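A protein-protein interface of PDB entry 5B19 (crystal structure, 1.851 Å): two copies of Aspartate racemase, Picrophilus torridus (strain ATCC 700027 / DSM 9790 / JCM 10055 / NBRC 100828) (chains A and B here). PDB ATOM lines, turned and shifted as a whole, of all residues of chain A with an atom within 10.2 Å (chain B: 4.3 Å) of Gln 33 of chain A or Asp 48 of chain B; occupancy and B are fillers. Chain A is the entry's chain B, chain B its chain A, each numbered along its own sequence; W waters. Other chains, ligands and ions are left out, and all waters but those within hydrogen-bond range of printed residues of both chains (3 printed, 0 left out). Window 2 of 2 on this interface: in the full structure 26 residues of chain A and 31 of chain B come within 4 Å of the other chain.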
ATOM      1  N   GLY A   2       1.906 -11.187   8.479  1.00  0.00           N
ATOM      2  CA  GLY A   2       1.849 -11.908   9.739  1.00  0.00           C
ATOM      3  C   GLY A   2       3.228 -12.137  10.329  1.00  0.00           C
ATOM      4  O   GLY A   2       4.255 -11.940   9.667  1.00  0.00           O
ATOM      5  N   LYS A   3       3.261 -12.538  11.594  1.00  0.00           N
ATOM      6  CA  LYS A   3       4.526 -12.798  12.270  1.00  0.00           C
ATOM      7  C   LYS A   3       4.976 -14.224  11.971  1.00  0.00           C
ATOM      8  O   LYS A   3       4.152 -15.134  11.938  1.00  0.00           O
ATOM      9  CB  LYS A   3       4.378 -12.600  13.781  1.00  0.00           C
ATOM     10  CG  LYS A   3       3.985 -11.183  14.192  1.00  0.00           C
ATOM     11  CD  LYS A   3       4.064 -11.000  15.709  1.00  0.00           C
ATOM     12  CE  LYS A   3       2.707 -10.614  16.295  1.00  0.00           C
ATOM     13  NZ  LYS A   3       1.691 -11.702  16.086  1.00  0.00           N
ATOM     14  N   THR A  27      -5.899 -23.502   8.484  1.00  0.00           N
ATOM     15  CA  THR A  27      -5.768 -22.083   8.160  1.00  0.00           C
ATOM     16  C   THR A  27      -6.754 -21.679   7.083  1.00  0.00           C
ATOM     17  O   THR A  27      -6.823 -22.296   6.018  1.00  0.00           O
ATOM     18  CB  THR A  27      -4.341 -21.735   7.688  1.00  0.00           C
ATOM     19  OG1 THR A  27      -3.395 -22.225   8.643  1.00  0.00           O
ATOM     20  CG2 THR A  27      -4.166 -20.223   7.524  1.00  0.00           C
ATOM     21  N   ASP A  28      -7.505 -20.628   7.380  1.00  0.00           N
ATOM     22  CA  ASP A  28      -8.459 -20.034   6.457  1.00  0.00           C
ATOM     23  C   ASP A  28      -7.735 -19.096   5.496  1.00  0.00           C
ATOM     24  O   ASP A  28      -7.422 -17.951   5.840  1.00  0.00           O
ATOM     25  CB  ASP A  28      -9.537 -19.282   7.229  1.00  0.00           C
ATOM     26  CG  ASP A  28     -10.606 -18.698   6.329  1.00  0.00           C
ATOM     27  OD1 ASP A  28     -10.678 -19.079   5.136  1.00  0.00           O
ATOM     28  OD2 ASP A  28     -11.384 -17.860   6.828  1.00  0.00           O
ATOM     29  N   ALA A  29      -7.482 -19.590   4.294  1.00  0.00           N
ATOM     30  CA  ALA A  29      -6.683 -18.867   3.320  1.00  0.00           C
ATOM     31  C   ALA A  29      -7.138 -19.205   1.926  1.00  0.00           C
ATOM     32  O   ALA A  29      -7.195 -20.378   1.554  1.00  0.00           O
ATOM     33  CB  ALA A  29      -5.207 -19.201   3.485  1.00  0.00           C
ATOM     34  N   GLU A  30      -7.454 -18.177   1.151  1.00  0.00           N
ATOM     35  CA  GLU A  30      -7.813 -18.376  -0.246  1.00  0.00           C
ATOM     36  C   GLU A  30      -6.621 -18.207  -1.187  1.00  0.00           C
ATOM     37  O   GLU A  30      -6.676 -18.633  -2.339  1.00  0.00           O
ATOM     38  CB  GLU A  30      -8.923 -17.417  -0.649  1.00  0.00           C
ATOM     39  CG  GLU A  30     -10.320 -17.931  -0.341  1.00  0.00           C
ATOM     40  CD  GLU A  30     -11.392 -17.055  -0.951  1.00  0.00           C
ATOM     41  OE1 GLU A  30     -11.353 -16.841  -2.184  1.00  0.00           O
ATOM     42  OE2 GLU A  30     -12.259 -16.562  -0.194  1.00  0.00           O
ATOM     43  N   ILE A  31      -5.555 -17.575  -0.699  1.00  0.00           N
ATOM     44  CA  ILE A  31      -4.318 -17.426  -1.470  1.00  0.00           C
ATOM     45  C   ILE A  31      -3.147 -17.861  -0.582  1.00  0.00           C
ATOM     46  O   ILE A  31      -3.266 -17.832   0.645  1.00  0.00           O
ATOM     47  CB  ILE A  31      -4.093 -15.966  -1.955  1.00  0.00           C
ATOM     48  CG1 ILE A  31      -4.105 -14.990  -0.774  1.00  0.00           C
ATOM     49  CG2 ILE A  31      -5.131 -15.561  -2.989  1.00  0.00           C
ATOM     50  CD1 ILE A  31      -3.705 -13.565  -1.149  1.00  0.00           C
ATOM     51  N   ASP A  32      -2.037 -18.272  -1.195  1.00  0.00           N
ATOM     52  CA  ASP A  32      -0.858 -18.715  -0.451  1.00  0.00           C
ATOM     53  C   ASP A  32      -0.459 -17.708   0.629  1.00  0.00           C
ATOM     54  O   ASP A  32      -0.047 -18.087   1.720  1.00  0.00           O
ATOM     55  CB  ASP A  32       0.354 -18.925  -1.382  1.00  0.00           C
ATOM     56  CG  ASP A  32       0.191 -20.096  -2.356  1.00  0.00           C
ATOM     57  OD1 ASP A  32      -0.717 -20.953  -2.182  1.00  0.00           O
ATOM     58  OD2 ASP A  32       1.027 -20.166  -3.295  1.00  0.00           O
ATOM     59  N   GLN A  33      -0.566 -16.424   0.322  1.00  0.00           N
ATOM     60  CA  GLN A  33       0.005 -15.400   1.188  1.00  0.00           C
ATOM     61  C   GLN A  33      -0.815 -15.202   2.467  1.00  0.00           C
ATOM     62  O   GLN A  33      -0.413 -14.457   3.351  1.00  0.00           O
ATOM     63  CB  GLN A  33       0.152 -14.071   0.425  1.00  0.00           C
ATOM     64  CG  GLN A  33       1.245 -14.053  -0.667  1.00  0.00           C
ATOM     65  CD  GLN A  33       0.917 -14.914  -1.880  1.00  0.00           C
ATOM     66  OE1 GLN A  33      -0.252 -15.123  -2.222  1.00  0.00           O
ATOM     67  NE2 GLN A  33       1.962 -15.439  -2.532  1.00  0.00           N
ATOM     68  N   ASP A  34      -1.933 -15.911   2.582  1.00  0.00           N
ATOM     69  CA  ASP A  34      -2.740 -15.860   3.800  1.00  0.00           C
ATOM     70  C   ASP A  34      -2.472 -17.043   4.737  1.00  0.00           C
ATOM     71  O   ASP A  34      -3.154 -17.217   5.749  1.00  0.00           O
ATOM     72  CB  ASP A  34      -4.216 -15.816   3.445  1.00  0.00           C
ATOM     73  CG  ASP A  34      -4.642 -14.460   2.909  1.00  0.00           C
ATOM     74  OD1 ASP A  34      -3.979 -13.454   3.250  1.00  0.00           O
ATOM     75  OD2 ASP A  34      -5.619 -14.408   2.137  1.00  0.00           O
ATOM     76  N   HIS A  35      -1.480 -17.851   4.399  1.00  0.00           N
ATOM     77  CA  HIS A  35      -1.101 -18.939   5.268  1.00  0.00           C
ATOM     78  C   HIS A  35      -0.071 -18.522   6.303  1.00  0.00           C
ATOM     79  O   HIS A  35       0.452 -17.405   6.296  1.00  0.00           O
ATOM     80  CB  HIS A  35      -0.579 -20.123   4.441  1.00  0.00           C
ATOM     81  CG  HIS A  35      -1.670 -20.965   3.862  1.00  0.00           C
ATOM     82  ND1 HIS A  35      -2.294 -21.957   4.584  1.00  0.00           N
ATOM     83  CD2 HIS A  35      -2.280 -20.934   2.653  1.00  0.00           C
ATOM     84  CE1 HIS A  35      -3.222 -22.526   3.831  1.00  0.00           C
ATOM     85  NE2 HIS A  35      -3.235 -21.923   2.659  1.00  0.00           N
ATOM     86  N   VAL A  36       0.242 -19.457   7.181  1.00  0.00           N
ATOM     87  CA  VAL A  36       1.104 -19.180   8.322  1.00  0.00           C
ATOM     88  C   VAL A  36       2.564 -19.234   7.937  1.00  0.00           C
ATOM     89  O   VAL A  36       3.007 -20.184   7.291  1.00  0.00           O
ATOM     90  CB  VAL A  36       0.838 -20.178   9.454  1.00  0.00           C
ATOM     91  CG1 VAL A  36       1.894 -20.047  10.554  1.00  0.00           C
ATOM     92  CG2 VAL A  36      -0.560 -19.960  10.009  1.00  0.00           C
ATOM     93  N   ARG A  37       3.302 -18.204   8.335  1.00  0.00           N
ATOM     94  CA  ARG A  37       4.737 -18.186   8.168  1.00  0.00           C
ATOM     95  C   ARG A  37       5.390 -18.873   9.354  1.00  0.00           C
ATOM     96  O   ARG A  37       5.161 -18.474  10.502  1.00  0.00           O
ATOM     97  CB  ARG A  37       5.251 -16.757   8.054  1.00  0.00           C
ATOM     98  CG  ARG A  37       4.489 -15.916   7.051  1.00  0.00           C
ATOM     99  CD  ARG A  37       4.925 -14.473   7.174  1.00  0.00           C
ATOM    100  NE  ARG A  37       6.174 -14.215   6.460  1.00  0.00           N
ATOM    101  CZ  ARG A  37       7.065 -13.295   6.821  1.00  0.00           C
ATOM    102  NH1 ARG A  37       6.850 -12.548   7.905  1.00  0.00           N
ATOM    103  NH2 ARG A  37       8.176 -13.124   6.108  1.00  0.00           N
ATOM    104  N   ALA A 219       0.370 -16.169  14.755  1.00  0.00           N
ATOM    105  CA  ALA A 219       0.940 -15.825  13.453  1.00  0.00           C
ATOM    106  C   ALA A 219       0.173 -14.683  12.789  1.00  0.00           C
ATOM    107  O   ALA A 219       0.542 -14.243  11.699  1.00  0.00           O
ATOM    108  CB  ALA A 219       0.946 -17.041  12.543  1.00  0.00           C
ATOM    109  N   GLY A 220      -0.903 -14.233  13.435  1.00  0.00           N
ATOM    110  CA  GLY A 220      -1.744 -13.175  12.899  1.00  0.00           C
ATOM    111  C   GLY A 220      -2.598 -13.664  11.749  1.00  0.00           C
ATOM    112  O   GLY A 220      -3.033 -12.888  10.897  1.00  0.00           O
ATOM    113  N   LYS A 221      -2.834 -14.967  11.707  1.00  0.00           N
ATOM    114  CA  LYS A 221      -3.602 -15.553  10.619  1.00  0.00           C
ATOM    115  C   LYS A 221      -4.998 -15.948  11.102  1.00  0.00           C
ATOM    116  O   LYS A 221      -5.306 -15.838  12.294  1.00  0.00           O
ATOM    117  CB  LYS A 221      -2.851 -16.758  10.025  1.00  0.00           C
ATOM    118  CG  LYS A 221      -1.482 -16.379   9.433  1.00  0.00           C
ATOM    119  CD  LYS A 221      -1.641 -15.357   8.293  1.00  0.00           C
ATOM    120  CE  LYS A 221      -0.290 -14.768   7.831  1.00  0.00           C
ATOM    121  NZ  LYS A 221      -0.210 -14.698   6.309  1.00  0.00           N
ATOM    122  N   ARG A 222      -5.837 -16.375  10.167  1.00  0.00           N
ATOM    123  CA  ARG A 222      -7.235 -16.703  10.454  1.00  0.00           C
ATOM    124  C   ARG A 222      -7.471 -18.210  10.596  1.00  0.00           C
ATOM    125  O   ARG A 222      -6.924 -19.013   9.843  1.00  0.00           O
ATOM    126  CB  ARG A 222      -8.144 -16.145   9.359  1.00  0.00           C
ATOM    127  CG  ARG A 222      -7.973 -14.664   9.097  1.00  0.00           C
ATOM    128  CD  ARG A 222      -8.976 -14.133   8.066  1.00  0.00           C
ATOM    129  NE  ARG A 222      -8.969 -14.900   6.816  1.00  0.00           N
ATOM    130  CZ  ARG A 222      -8.256 -14.590   5.731  1.00  0.00           C
ATOM    131  NH1 ARG A 222      -7.470 -13.517   5.719  1.00  0.00           N
ATOM    132  NH2 ARG A 222      -8.326 -15.361   4.650  1.00  0.00           N
ATOM    133  N   PRO B  44       4.981 -18.425   3.253  1.00  0.00           N
ATOM    134  CA  PRO B  44       4.000 -18.282   2.175  1.00  0.00           C
ATOM    135  C   PRO B  44       3.708 -16.832   1.797  1.00  0.00           C
ATOM    136  O   PRO B  44       3.019 -16.617   0.808  1.00  0.00           O
ATOM    137  CB  PRO B  44       2.744 -18.960   2.744  1.00  0.00           C
ATOM    138  CG  PRO B  44       2.933 -18.959   4.229  1.00  0.00           C
ATOM    139  CD  PRO B  44       4.408 -19.023   4.475  1.00  0.00           C
ATOM    140  N   GLU B  45       4.217 -15.859   2.550  1.00  0.00           N
ATOM    141  CA  GLU B  45       4.047 -14.472   2.140  1.00  0.00           C
ATOM    142  C   GLU B  45       5.127 -14.064   1.134  1.00  0.00           C
ATOM    143  O   GLU B  45       5.172 -12.918   0.710  1.00  0.00           O
ATOM    144  CB  GLU B  45       4.054 -13.519   3.350  1.00  0.00           C
ATOM    145  CG  GLU B  45       2.921 -13.787   4.315  1.00  0.00           C
ATOM    146  CD  GLU B  45       2.718 -12.677   5.353  1.00  0.00           C
ATOM    147  OE1 GLU B  45       3.384 -11.623   5.281  1.00  0.00           O
ATOM    148  OE2 GLU B  45       1.896 -12.880   6.262  1.00  0.00           O
ATOM    149  N   ILE B  46       5.998 -14.993   0.750  1.00  0.00           N
ATOM    150  CA  ILE B  46       6.798 -14.757  -0.450  1.00  0.00           C
ATOM    151  C   ILE B  46       5.838 -14.354  -1.577  1.00  0.00           C
ATOM    152  O   ILE B  46       4.825 -15.016  -1.805  1.00  0.00           O
ATOM    153  CB  ILE B  46       7.618 -16.000  -0.857  1.00  0.00           C
ATOM    154  CG1 ILE B  46       8.747 -16.233   0.141  1.00  0.00           C
ATOM    155  CG2 ILE B  46       8.188 -15.840  -2.286  1.00  0.00           C
ATOM    156  CD1 ILE B  46       9.357 -17.623   0.053  1.00  0.00           C
ATOM    157  N   PRO B  47       6.124 -13.234  -2.263  1.00  0.00           N
ATOM    158  CA  PRO B  47       5.169 -12.711  -3.247  1.00  0.00           C
ATOM    159  C   PRO B  47       4.817 -13.710  -4.343  1.00  0.00           C
ATOM    160  O   PRO B  47       5.675 -14.499  -4.735  1.00  0.00           O
ATOM    161  CB  PRO B  47       5.896 -11.503  -3.862  1.00  0.00           C
ATOM    162  CG  PRO B  47       6.995 -11.155  -2.911  1.00  0.00           C
ATOM    163  CD  PRO B  47       7.315 -12.384  -2.097  1.00  0.00           C
ATOM    164  N   ASP B  48       3.581 -13.653  -4.828  1.00  0.00           N
ATOM    165  CA  ASP B  48       3.121 -14.534  -5.911  1.00  0.00           C
ATOM    166  C   ASP B  48       4.086 -14.528  -7.084  1.00  0.00           C
ATOM    167  O   ASP B  48       4.382 -13.463  -7.640  1.00  0.00           O
ATOM    168  CB  ASP B  48       1.751 -14.100  -6.413  1.00  0.00           C
ATOM    169  CG  ASP B  48       1.115 -15.122  -7.345  1.00  0.00           C
ATOM    170  OD1 ASP B  48       0.221 -15.857  -6.888  1.00  0.00           O
ATOM    171  OD2 ASP B  48       1.466 -15.165  -8.534  1.00  0.00           O
ATOM    172  N   ARG B  49       4.546 -15.709  -7.483  1.00  0.00           N
ATOM    173  CA  ARG B  49       5.583 -15.757  -8.497  1.00  0.00           C
ATOM    174  C   ARG B  49       5.045 -15.555  -9.921  1.00  0.00           C
ATOM    175  O   ARG B  49       5.749 -15.006 -10.758  1.00  0.00           O
ATOM    176  CB  ARG B  49       6.374 -17.049  -8.281  1.00  0.00           C
ATOM    177  CG  ARG B  49       6.926 -16.897  -6.849  1.00  0.00           C
ATOM    178  CD  ARG B  49       7.017 -18.119  -6.076  1.00  0.00           C
ATOM    179  NE  ARG B  49       5.757 -18.733  -5.647  1.00  0.00           N
ATOM    180  CZ  ARG B  49       4.960 -18.369  -4.644  1.00  0.00           C
ATOM    181  NH1 ARG B  49       3.911 -19.134  -4.395  1.00  0.00           N
ATOM    182  NH2 ARG B  49       5.172 -17.287  -3.896  1.00  0.00           N
ATOM    183  N   ILE B  50       3.777 -15.888 -10.173  1.00  0.00           N
ATOM    184  CA  ILE B  50       3.184 -15.612 -11.485  1.00  0.00           C
ATOM    185  C   ILE B  50       2.957 -14.108 -11.705  1.00  0.00           C
ATOM    186  O   ILE B  50       3.198 -13.597 -12.804  1.00  0.00           O
ATOM    187  CB  ILE B  50       1.849 -16.367 -11.674  1.00  0.00           C
ATOM    188  CG1 ILE B  50       2.014 -17.843 -11.272  1.00  0.00           C
ATOM    189  CG2 ILE B  50       1.301 -16.188 -13.097  1.00  0.00           C
ATOM    190  CD1 ILE B  50       3.122 -18.589 -12.043  1.00  0.00           C
ATOM    191  N   GLU B  51       2.518 -13.400 -10.663  1.00  0.00           N
ATOM    192  CA  GLU B  51       2.342 -11.943 -10.754  1.00  0.00           C
ATOM    193  C   GLU B  51       3.679 -11.247 -10.900  1.00  0.00           C
ATOM    194  O   GLU B  51       3.779 -10.224 -11.580  1.00  0.00           O
ATOM    195  CB  GLU B  51       1.621 -11.401  -9.523  1.00  0.00           C
ATOM    196  CG  GLU B  51       0.143 -11.811  -9.485  1.00  0.00           C
ATOM    197  CD  GLU B  51      -0.577 -11.354  -8.224  1.00  0.00           C
ATOM    198  OE1 GLU B  51       0.024 -10.632  -7.390  1.00  0.00           O
ATOM    199  OE2 GLU B  51      -1.761 -11.717  -8.065  1.00  0.00           O
ATOM    200  N   ALA B  52       4.690 -11.788 -10.233  1.00  0.00           N
ATOM    201  CA  ALA B  52       6.041 -11.246 -10.333  1.00  0.00           C
ATOM    202  C   ALA B  52       6.530 -11.379 -11.762  1.00  0.00           C
ATOM    203  O   ALA B  52       7.119 -10.447 -12.318  1.00  0.00           O
ATOM    204  CB  ALA B  52       6.985 -11.952  -9.385  1.00  0.00           C
HETATM  205  O   HOH W   1       3.824  -9.752   7.054  1.00  0.00           O
HETATM  206  O   HOH W   2       3.709 -18.189  -1.359  1.00  0.00           O
HETATM  207  O   HOH W   3       1.454 -17.404  -4.498  1.00  0.00           O
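Of the 9 printed residues of chain B, 6 touch a printed residue of chain A.
Along chain B the printed residues that touch a printed residue of chain A span positions 44 to 49.
Among the printed residues, Asp or Glu carboxylates within 4 Å of a Lys or Arg side-chain nitrogen of the other chain: Asp 32 of chain A with Arg 49 of chain B (3.3 Å), Arg 37 of chain A with Glu 45 of chain B (3.99 Å) and Lys 221 of chain A with Glu 45 of chain B (2.8 Å).
Of chain B, only Pro 44 (3.3 Å), Glu 45 (3.5 Å), Ile 46 (3.0 Å), Pro 47 (3.8 Å), Asp 48 (3.3 Å) and Arg 49 (3.9 Å) come within 4 Å of Gln 33 of chain A.
Printed residues of chain A within 4 Å of Asp 48 of chain B: Gln 33.
Of chain A, only Gly 2 (2.8 Å), Gln 33 (3.5 Å), Arg 37 (3.4 Å) and Lys 221 (2.8 Å) come within 4 Å of Glu 45 of chain B.
Of chain A, only Gln 33 (3.8 Å) comes within 4 Å of Pro 47 of chain B.
Arg 49 of chain B touches just these residues of chain A: Asp 32 and Gln 33.
Ile 50 of chain B touches none of the printed residues of chain A.
No residue of chain A comes within 4 Å of Glu 51 of chain B.
Of the printed residues of chain A, Pro 44 of chain B touches Asp 32 (3.1 Å), Gln 33 (3.3 Å), His 35 (3.6 Å), Val 36 (3.3 Å) and Arg 37 (3.8 Å).
Of the printed residues of chain B, Val 36 of chain A touches Pro 44 (3.3 Å).
Of the printed residues of chain B, Lys 221 of chain A touches Glu 45.
Of the printed residues of chain A, Ile 46 of chain B touches Gln 33 (3.0 Å).
Ala 219 of chain A touches none of the printed residues of chain B.
Ile 31 of chain A touches none of the printed residues of chain B.
Among the printed residues, merely in contact across the chains: Asp 32 of chain A with Pro 44 of chain B, Gln 33 of chain A with Pro 44 of chain B, Gln 33 of chain A with Glu 45 of chain B, Gln 33 of chain A with Pro 47 of chain B, Gln 33 of chain A with Arg 49 of chain B, His 35 of chain A with Pro 44 of chain B, Val 36 of chain A with Pro 44 of chain B and Arg 37 of chain A with Pro 44 of chain B.
NH2 of Arg 49 of chain B sits at hydrogen-bond distance from O of Ile 46 of chain B, at 3.1 Å.
O of Pro 47 of chain B sits at hydrogen-bond distance from NH2 of Arg 49 of chain B, 3.0 Å away.
The backbone NH of Ile 50 of chain B sits at hydrogen-bond distance from the side-chain carboxylate of Asp 48 of chain B, at 2.9 Å.
The guanidinium group (NH1) of Arg 37 of chain A lies within hydrogen-bond range of the backbone carbonyl oxygen (O) of Gly 2 of chain A (3.2 Å).
The backbone carbonyl oxygen of Gln 33 of chain A sits at hydrogen-bond distance from the side-chain amino group of Lys 221 of chain A (3.0 Å).
The side-chain amino group (NZ) of Lys 221 of chain A lies within hydrogen-bond range of the backbone carbonyl oxygen (O) of His 35 of chain A, at 2.8 Å.
Water W1 lies within hydrogen-bond range of the side-chain carboxylate of Glu 45 of chain B and the backbone NH of Gly 2 of chain A.
Water W2 lies within hydrogen-bond range of O of Pro 44 of chain B (2.8 Å), NH2 of Arg 49 of chain B (3.1 Å), O of Ile 46 of chain B (3.4 Å) and NE2 of Gln 33 of chain A (3.5 Å).
Water W3 lies within hydrogen-bond range of NE2 of Gln 33 of chain A (2.8 Å), NH1 of Arg 49 of chain B (3.0 Å), OD2 of Asp 32 of chain A (3.0 Å) and OD1 of Asp 48 of chain B (3.1 Å).
No position is printed for both chains.
Of the 14 pairs that touch across the chains among the printed residues, none has its exchanged pair printed and touching as well.
The side-chain carboxylate (OE2) of Glu 45 of chain B lies within hydrogen-bond range of the backbone NH (N) of Gly 2 of chain A (2.8 Å).
OE1 of Glu 45 of chain B is in salt-bridge range of NE of Arg 37 of chain A, 3.99 Å away.
The side-chain carboxylate (OE2) of Glu 45 of chain B is in salt-bridge range of the side-chain amino group (NZ) of Lys 221 of chain A (2.8 Å).
The backbone carbonyl oxygen (O) of Ile 46 of chain B sits at hydrogen-bond distance from the side-chain amide nitrogen (NE2) of Gln 33 of chain A (3.0 Å).
The side-chain amide nitrogen of Gln 33 of chain A sits close to the backbone NH of Asp 48 of chain B, at 3.3 Å.
OD2 of Asp 32 of chain A lies within salt-bridge range of NH1 of Arg 49 of chain B (3.3 Å).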
